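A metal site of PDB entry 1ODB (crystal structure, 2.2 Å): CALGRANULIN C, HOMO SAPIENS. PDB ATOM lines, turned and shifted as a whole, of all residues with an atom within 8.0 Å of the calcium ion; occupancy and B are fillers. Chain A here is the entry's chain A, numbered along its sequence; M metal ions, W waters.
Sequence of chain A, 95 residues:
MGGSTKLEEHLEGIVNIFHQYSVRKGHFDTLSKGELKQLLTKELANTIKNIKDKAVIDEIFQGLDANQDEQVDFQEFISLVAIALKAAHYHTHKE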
ATOM      1  N   PHE A  18      34.264 -34.138  -3.038  1.00  0.00           N
ATOM      2  CA  PHE A  18      33.437 -32.953  -2.816  1.00  0.00           C
ATOM      3  C   PHE A  18      32.632 -32.556  -4.048  1.00  0.00           C
ATOM      4  O   PHE A  18      31.454 -32.236  -3.959  1.00  0.00           O
ATOM      5  CB  PHE A  18      34.329 -31.762  -2.413  1.00  0.00           C
ATOM      6  CG  PHE A  18      33.603 -30.454  -2.327  1.00  0.00           C
ATOM      7  CD1 PHE A  18      32.989 -30.054  -1.145  1.00  0.00           C
ATOM      8  CD2 PHE A  18      33.554 -29.600  -3.424  1.00  0.00           C
ATOM      9  CE1 PHE A  18      32.312 -28.818  -1.084  1.00  0.00           C
ATOM     10  CE2 PHE A  18      32.889 -28.393  -3.364  1.00  0.00           C
ATOM     11  CZ  PHE A  18      32.284 -27.982  -2.199  1.00  0.00           C
ATOM     12  N   HIS A  19      33.282 -32.574  -5.211  1.00  0.00           N
ATOM     13  CA  HIS A  19      32.622 -32.226  -6.474  1.00  0.00           C
ATOM     14  C   HIS A  19      31.587 -33.226  -6.946  1.00  0.00           C
ATOM     15  O   HIS A  19      30.591 -32.845  -7.552  1.00  0.00           O
ATOM     16  CB  HIS A  19      33.664 -31.987  -7.564  1.00  0.00           C
ATOM     17  CG  HIS A  19      34.527 -30.811  -7.302  1.00  0.00           C
ATOM     18  ND1 HIS A  19      35.630 -30.868  -6.479  1.00  0.00           N
ATOM     19  CD2 HIS A  19      34.436 -29.521  -7.730  1.00  0.00           C
ATOM     20  CE1 HIS A  19      36.187 -29.674  -6.417  1.00  0.00           C
ATOM     21  NE2 HIS A  19      35.487 -28.841  -7.154  1.00  0.00           N
ATOM     22  N   TYR A  21      29.540 -34.669  -5.121  1.00  0.00           N
ATOM     23  CA  TYR A  21      28.328 -34.316  -4.368  1.00  0.00           C
ATOM     24  C   TYR A  21      27.820 -32.875  -4.621  1.00  0.00           C
ATOM     25  O   TYR A  21      26.635 -32.652  -4.684  1.00  0.00           O
ATOM     26  CB  TYR A  21      28.509 -34.665  -2.867  1.00  0.00           C
ATOM     27  CG  TYR A  21      28.576 -36.173  -2.678  1.00  0.00           C
ATOM     28  CD1 TYR A  21      27.419 -36.914  -2.484  1.00  0.00           C
ATOM     29  CD2 TYR A  21      29.799 -36.858  -2.704  1.00  0.00           C
ATOM     30  CE1 TYR A  21      27.462 -38.300  -2.345  1.00  0.00           C
ATOM     31  CE2 TYR A  21      29.859 -38.244  -2.562  1.00  0.00           C
ATOM     32  CZ  TYR A  21      28.699 -38.958  -2.382  1.00  0.00           C
ATOM     33  OH  TYR A  21      28.757 -40.349  -2.227  1.00  0.00           O
ATOM     34  N   SER A  22      28.741 -31.940  -4.883  1.00  0.00           N
ATOM     35  CA  SER A  22      28.422 -30.524  -5.013  1.00  0.00           C
ATOM     36  C   SER A  22      27.747 -30.125  -6.321  1.00  0.00           C
ATOM     37  O   SER A  22      27.020 -29.105  -6.373  1.00  0.00           O
ATOM     38  CB  SER A  22      29.654 -29.633  -4.793  1.00  0.00           C
ATOM     39  OG  SER A  22      30.568 -29.669  -5.893  1.00  0.00           O
ATOM     40  N   VAL A  23      27.946 -30.930  -7.353  1.00  0.00           N
ATOM     41  CA  VAL A  23      27.341 -30.667  -8.676  1.00  0.00           C
ATOM     42  C   VAL A  23      25.873 -31.125  -8.784  1.00  0.00           C
ATOM     43  O   VAL A  23      25.183 -30.857  -9.807  1.00  0.00           O
ATOM     44  CB  VAL A  23      28.147 -31.328  -9.815  1.00  0.00           C
ATOM     45  CG1 VAL A  23      29.617 -30.816  -9.817  1.00  0.00           C
ATOM     46  CG2 VAL A  23      28.077 -32.895  -9.763  1.00  0.00           C
ATOM     47  N   ARG A  24      25.377 -31.771  -7.727  1.00  0.00           N
ATOM     48  CA  ARG A  24      24.130 -32.527  -7.869  1.00  0.00           C
ATOM     49  C   ARG A  24      22.887 -31.670  -7.981  1.00  0.00           C
ATOM     50  O   ARG A  24      22.023 -31.964  -8.816  1.00  0.00           O
ATOM     51  CB  ARG A  24      23.993 -33.544  -6.736  1.00  0.00           C
ATOM     52  CG  ARG A  24      24.955 -34.687  -6.918  1.00  0.00           C
ATOM     53  CD  ARG A  24      24.926 -35.726  -5.836  1.00  0.00           C
ATOM     54  NE  ARG A  24      25.917 -36.756  -6.070  1.00  0.00           N
ATOM     55  CZ  ARG A  24      25.886 -37.949  -5.527  1.00  0.00           C
ATOM     56  NH1 ARG A  24      24.912 -38.288  -4.716  1.00  0.00           N
ATOM     57  NH2 ARG A  24      26.841 -38.833  -5.798  1.00  0.00           N
ATOM     58  N   LYS A  25      22.816 -30.625  -7.159  1.00  0.00           N
ATOM     59  CA  LYS A  25      21.729 -29.637  -7.163  1.00  0.00           C
ATOM     60  C   LYS A  25      22.263 -28.219  -6.929  1.00  0.00           C
ATOM     61  O   LYS A  25      23.371 -28.019  -6.415  1.00  0.00           O
ATOM     62  CB  LYS A  25      20.558 -29.991  -6.162  1.00  0.00           C
ATOM     63  CG  LYS A  25      20.666 -29.511  -4.663  1.00  0.00           C
ATOM     64  CD  LYS A  25      19.263 -29.397  -3.849  1.00  0.00           C
ATOM     65  CE  LYS A  25      19.236 -30.128  -2.383  1.00  0.00           C
ATOM     66  NZ  LYS A  25      19.054 -29.335  -1.031  1.00  0.00           N
ATOM     67  N   GLY A  26      21.481 -27.239  -7.365  1.00  0.00           N
ATOM     68  CA  GLY A  26      21.781 -25.837  -7.171  1.00  0.00           C
ATOM     69  C   GLY A  26      23.183 -25.498  -7.632  1.00  0.00           C
ATOM     70  O   GLY A  26      23.655 -26.035  -8.645  1.00  0.00           O
ATOM     71  N   HIS A  27      23.842 -24.619  -6.889  1.00  0.00           N
ATOM     72  CA  HIS A  27      25.219 -24.215  -7.224  1.00  0.00           C
ATOM     73  C   HIS A  27      26.140 -25.425  -7.308  1.00  0.00           C
ATOM     74  O   HIS A  27      26.070 -26.341  -6.493  1.00  0.00           O
ATOM     75  CB  HIS A  27      25.760 -23.185  -6.208  1.00  0.00           C
ATOM     76  CG  HIS A  27      25.033 -21.879  -6.222  1.00  0.00           C
ATOM     77  ND1 HIS A  27      24.541 -21.312  -7.373  1.00  0.00           N
ATOM     78  CD2 HIS A  27      24.699 -21.042  -5.217  1.00  0.00           C
ATOM     79  CE1 HIS A  27      23.936 -20.178  -7.086  1.00  0.00           C
ATOM     80  NE2 HIS A  27      24.022 -19.988  -5.783  1.00  0.00           N
ATOM     81  N   PHE A  28      27.019 -25.426  -8.295  1.00  0.00           N
ATOM     82  CA  PHE A  28      27.882 -26.567  -8.585  1.00  0.00           C
ATOM     83  C   PHE A  28      29.139 -26.549  -7.692  1.00  0.00           C
ATOM     84  O   PHE A  28      29.798 -27.547  -7.575  1.00  0.00           O
ATOM     85  CB  PHE A  28      28.251 -26.595 -10.069  1.00  0.00           C
ATOM     86  CG  PHE A  28      27.062 -26.746 -10.999  1.00  0.00           C
ATOM     87  CD1 PHE A  28      26.420 -27.952 -11.120  1.00  0.00           C
ATOM     88  CD2 PHE A  28      26.580 -25.662 -11.711  1.00  0.00           C
ATOM     89  CE1 PHE A  28      25.321 -28.092 -11.961  1.00  0.00           C
ATOM     90  CE2 PHE A  28      25.462 -25.792 -12.545  1.00  0.00           C
ATOM     91  CZ  PHE A  28      24.837 -27.013 -12.660  1.00  0.00           C
ATOM     92  N   ASP A  29      29.427 -25.399  -7.074  1.00  0.00           N
ATOM     93  CA  ASP A  29      30.614 -25.219  -6.225  1.00  0.00           C
ATOM     94  C   ASP A  29      30.351 -25.413  -4.706  1.00  0.00           C
ATOM     95  O   ASP A  29      31.276 -25.265  -3.915  1.00  0.00           O
ATOM     96  CB  ASP A  29      31.318 -23.858  -6.495  1.00  0.00           C
ATOM     97  CG  ASP A  29      30.441 -22.641  -6.186  1.00  0.00           C
ATOM     98  OD1 ASP A  29      29.202 -22.730  -6.245  1.00  0.00           O
ATOM     99  OD2 ASP A  29      30.926 -21.515  -5.909  1.00  0.00           O
ATOM    100  N   THR A  30      29.119 -25.744  -4.319  1.00  0.00           N
ATOM    101  CA  THR A  30      28.775 -25.886  -2.902  1.00  0.00           C
ATOM    102  C   THR A  30      27.786 -27.013  -2.648  1.00  0.00           C
ATOM    103  O   THR A  30      27.056 -27.437  -3.532  1.00  0.00           O
ATOM    104  CB  THR A  30      28.190 -24.593  -2.299  1.00  0.00           C
ATOM    105  OG1 THR A  30      26.989 -24.271  -2.986  1.00  0.00           O
ATOM    106  CG2 THR A  30      29.099 -23.333  -2.510  1.00  0.00           C
ATOM    107  N   LEU A  31      27.778 -27.472  -1.398  1.00  0.00           N
ATOM    108  CA  LEU A  31      26.875 -28.528  -0.949  1.00  0.00           C
ATOM    109  C   LEU A  31      25.686 -27.913  -0.255  1.00  0.00           C
ATOM    110  O   LEU A  31      25.850 -27.223   0.759  1.00  0.00           O
ATOM    111  CB  LEU A  31      27.587 -29.431   0.062  1.00  0.00           C
ATOM    112  CG  LEU A  31      28.898 -30.084  -0.350  1.00  0.00           C
ATOM    113  CD1 LEU A  31      29.668 -30.605   0.860  1.00  0.00           C
ATOM    114  CD2 LEU A  31      28.640 -31.229  -1.322  1.00  0.00           C
ATOM    115  N   SER A  32      24.471 -28.158  -0.766  1.00  0.00           N
ATOM    116  CA  SER A  32      23.264 -27.968   0.042  1.00  0.00           C
ATOM    117  C   SER A  32      23.243 -28.976   1.184  1.00  0.00           C
ATOM    118  O   SER A  32      24.095 -29.864   1.246  1.00  0.00           O
ATOM    119  CB  SER A  32      21.989 -28.128  -0.800  1.00  0.00           C
ATOM    120  OG  SER A  32      21.980 -29.422  -1.423  1.00  0.00           O
ATOM    121  N   LYS A  33      22.252 -28.867   2.053  1.00  0.00           N
ATOM    122  CA  LYS A  33      22.091 -29.808   3.165  1.00  0.00           C
ATOM    123  C   LYS A  33      21.801 -31.210   2.628  1.00  0.00           C
ATOM    124  O   LYS A  33      22.326 -32.187   3.135  1.00  0.00           O
ATOM    125  CB  LYS A  33      20.987 -29.361   4.133  1.00  0.00           C
ATOM    126  CG  LYS A  33      20.693 -30.394   5.256  1.00  0.00           C
ATOM    127  CD  LYS A  33      20.235 -29.769   6.588  1.00  0.00           C
ATOM    128  CE  LYS A  33      18.994 -28.949   6.424  1.00  0.00           C
ATOM    129  NZ  LYS A  33      18.562 -28.282   7.715  1.00  0.00           N
ATOM    130  N   GLU A  35      22.741 -32.465  -0.316  1.00  0.00           N
ATOM    131  CA  GLU A  35      23.977 -32.991  -0.855  1.00  0.00           C
ATOM    132  C   GLU A  35      24.962 -33.421   0.235  1.00  0.00           C
ATOM    133  O   GLU A  35      25.618 -34.435   0.086  1.00  0.00           O
ATOM    134  CB  GLU A  35      24.673 -31.958  -1.762  1.00  0.00           C
ATOM    135  CG  GLU A  35      23.902 -31.655  -3.031  1.00  0.00           C
ATOM    136  CD  GLU A  35      24.445 -30.453  -3.794  1.00  0.00           C
ATOM    137  OE1 GLU A  35      24.802 -29.447  -3.156  1.00  0.00           O
ATOM    138  OE2 GLU A  35      24.533 -30.498  -5.035  1.00  0.00           O
ATOM    139  N   LEU A  36      25.058 -32.658   1.318  1.00  0.00           N
ATOM    140  CA  LEU A  36      25.898 -33.040   2.440  1.00  0.00           C
ATOM    141  C   LEU A  36      25.350 -34.324   3.049  1.00  0.00           C
ATOM    142  O   LEU A  36      26.094 -35.228   3.369  1.00  0.00           O
ATOM    143  CB  LEU A  36      25.918 -31.946   3.503  1.00  0.00           C
ATOM    144  CG  LEU A  36      26.730 -32.266   4.765  1.00  0.00           C
ATOM    145  CD1 LEU A  36      28.239 -32.360   4.413  1.00  0.00           C
ATOM    146  CD2 LEU A  36      26.477 -31.203   5.776  1.00  0.00           C
ATOM    147  N   GLN A  71      24.769 -23.106   2.439  1.00  0.00           N
ATOM    148  CA  GLN A  71      25.598 -23.835   1.500  1.00  0.00           C
ATOM    149  C   GLN A  71      26.883 -24.158   2.248  1.00  0.00           C
ATOM    150  O   GLN A  71      27.372 -23.339   3.015  1.00  0.00           O
ATOM    151  CB  GLN A  71      25.949 -22.956   0.292  1.00  0.00           C
ATOM    152  CG  GLN A  71      24.758 -22.581  -0.588  1.00  0.00           C
ATOM    153  CD  GLN A  71      24.135 -23.799  -1.244  1.00  0.00           C
ATOM    154  OE1 GLN A  71      24.841 -24.764  -1.650  1.00  0.00           O
ATOM    155  NE2 GLN A  71      22.810 -23.772  -1.367  1.00  0.00           N
ATOM    156  N   VAL A  72      27.437 -25.345   2.015  1.00  0.00           N
ATOM    157  CA  VAL A  72      28.765 -25.663   2.504  1.00  0.00           C
ATOM    158  C   VAL A  72      29.724 -25.556   1.328  1.00  0.00           C
ATOM    159  O   VAL A  72      29.674 -26.379   0.422  1.00  0.00           O
ATOM    160  CB  VAL A  72      28.829 -27.038   3.149  1.00  0.00           C
ATOM    161  CG1 VAL A  72      30.304 -27.416   3.449  1.00  0.00           C
ATOM    162  CG2 VAL A  72      27.953 -27.044   4.439  1.00  0.00           C
HETATM  163 CA    CA M   1      25.342 -28.049  -5.071  1.00  0.00          CA
HETATM  164  O   HOH W   1      24.295 -26.366  -3.776  1.00  0.00           O
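NZ of Lys 25 lies within hydrogen-bond range of OG of Ser 32 (3.0 Å).
The backbone carbonyl oxygen of Phe 18 lies close to the side-chain hydroxyl of Ser 22 (3.3 Å).
The backbone NH of Glu 35 lies within hydrogen-bond range of the side-chain hydroxyl of Ser 32 (3.3 Å).
The backbone carbonyl oxygen (O) of Phe 28 sits at hydrogen-bond distance from the side-chain hydroxyl (OG) of Ser 22, 2.8 Å away.
The side-chain carboxylate (OE2) of Glu 35 sits close to the backbone NH (N) of Arg 24.
The side-chain hydroxyl (OG1) of Thr 30 sits at hydrogen-bond distance from the side-chain amide oxygen (OE1) of Gln 71.
The nearest printed residue that does not touch the calcium ion is Gly 26 (4.2 Å).
The calcium ion is bound by O of His 27 (2.3 Å), water W1 (2.4 Å), O of Ser 22 (2.4 Å), O of Thr 30 (2.4 Å), O of Lys 25 (2.4 Å), OE1 of Glu 35 (2.4 Å) and OE2 of Glu 35 (2.6 Å).
The calcium ion has seven donor atoms within binding distance.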
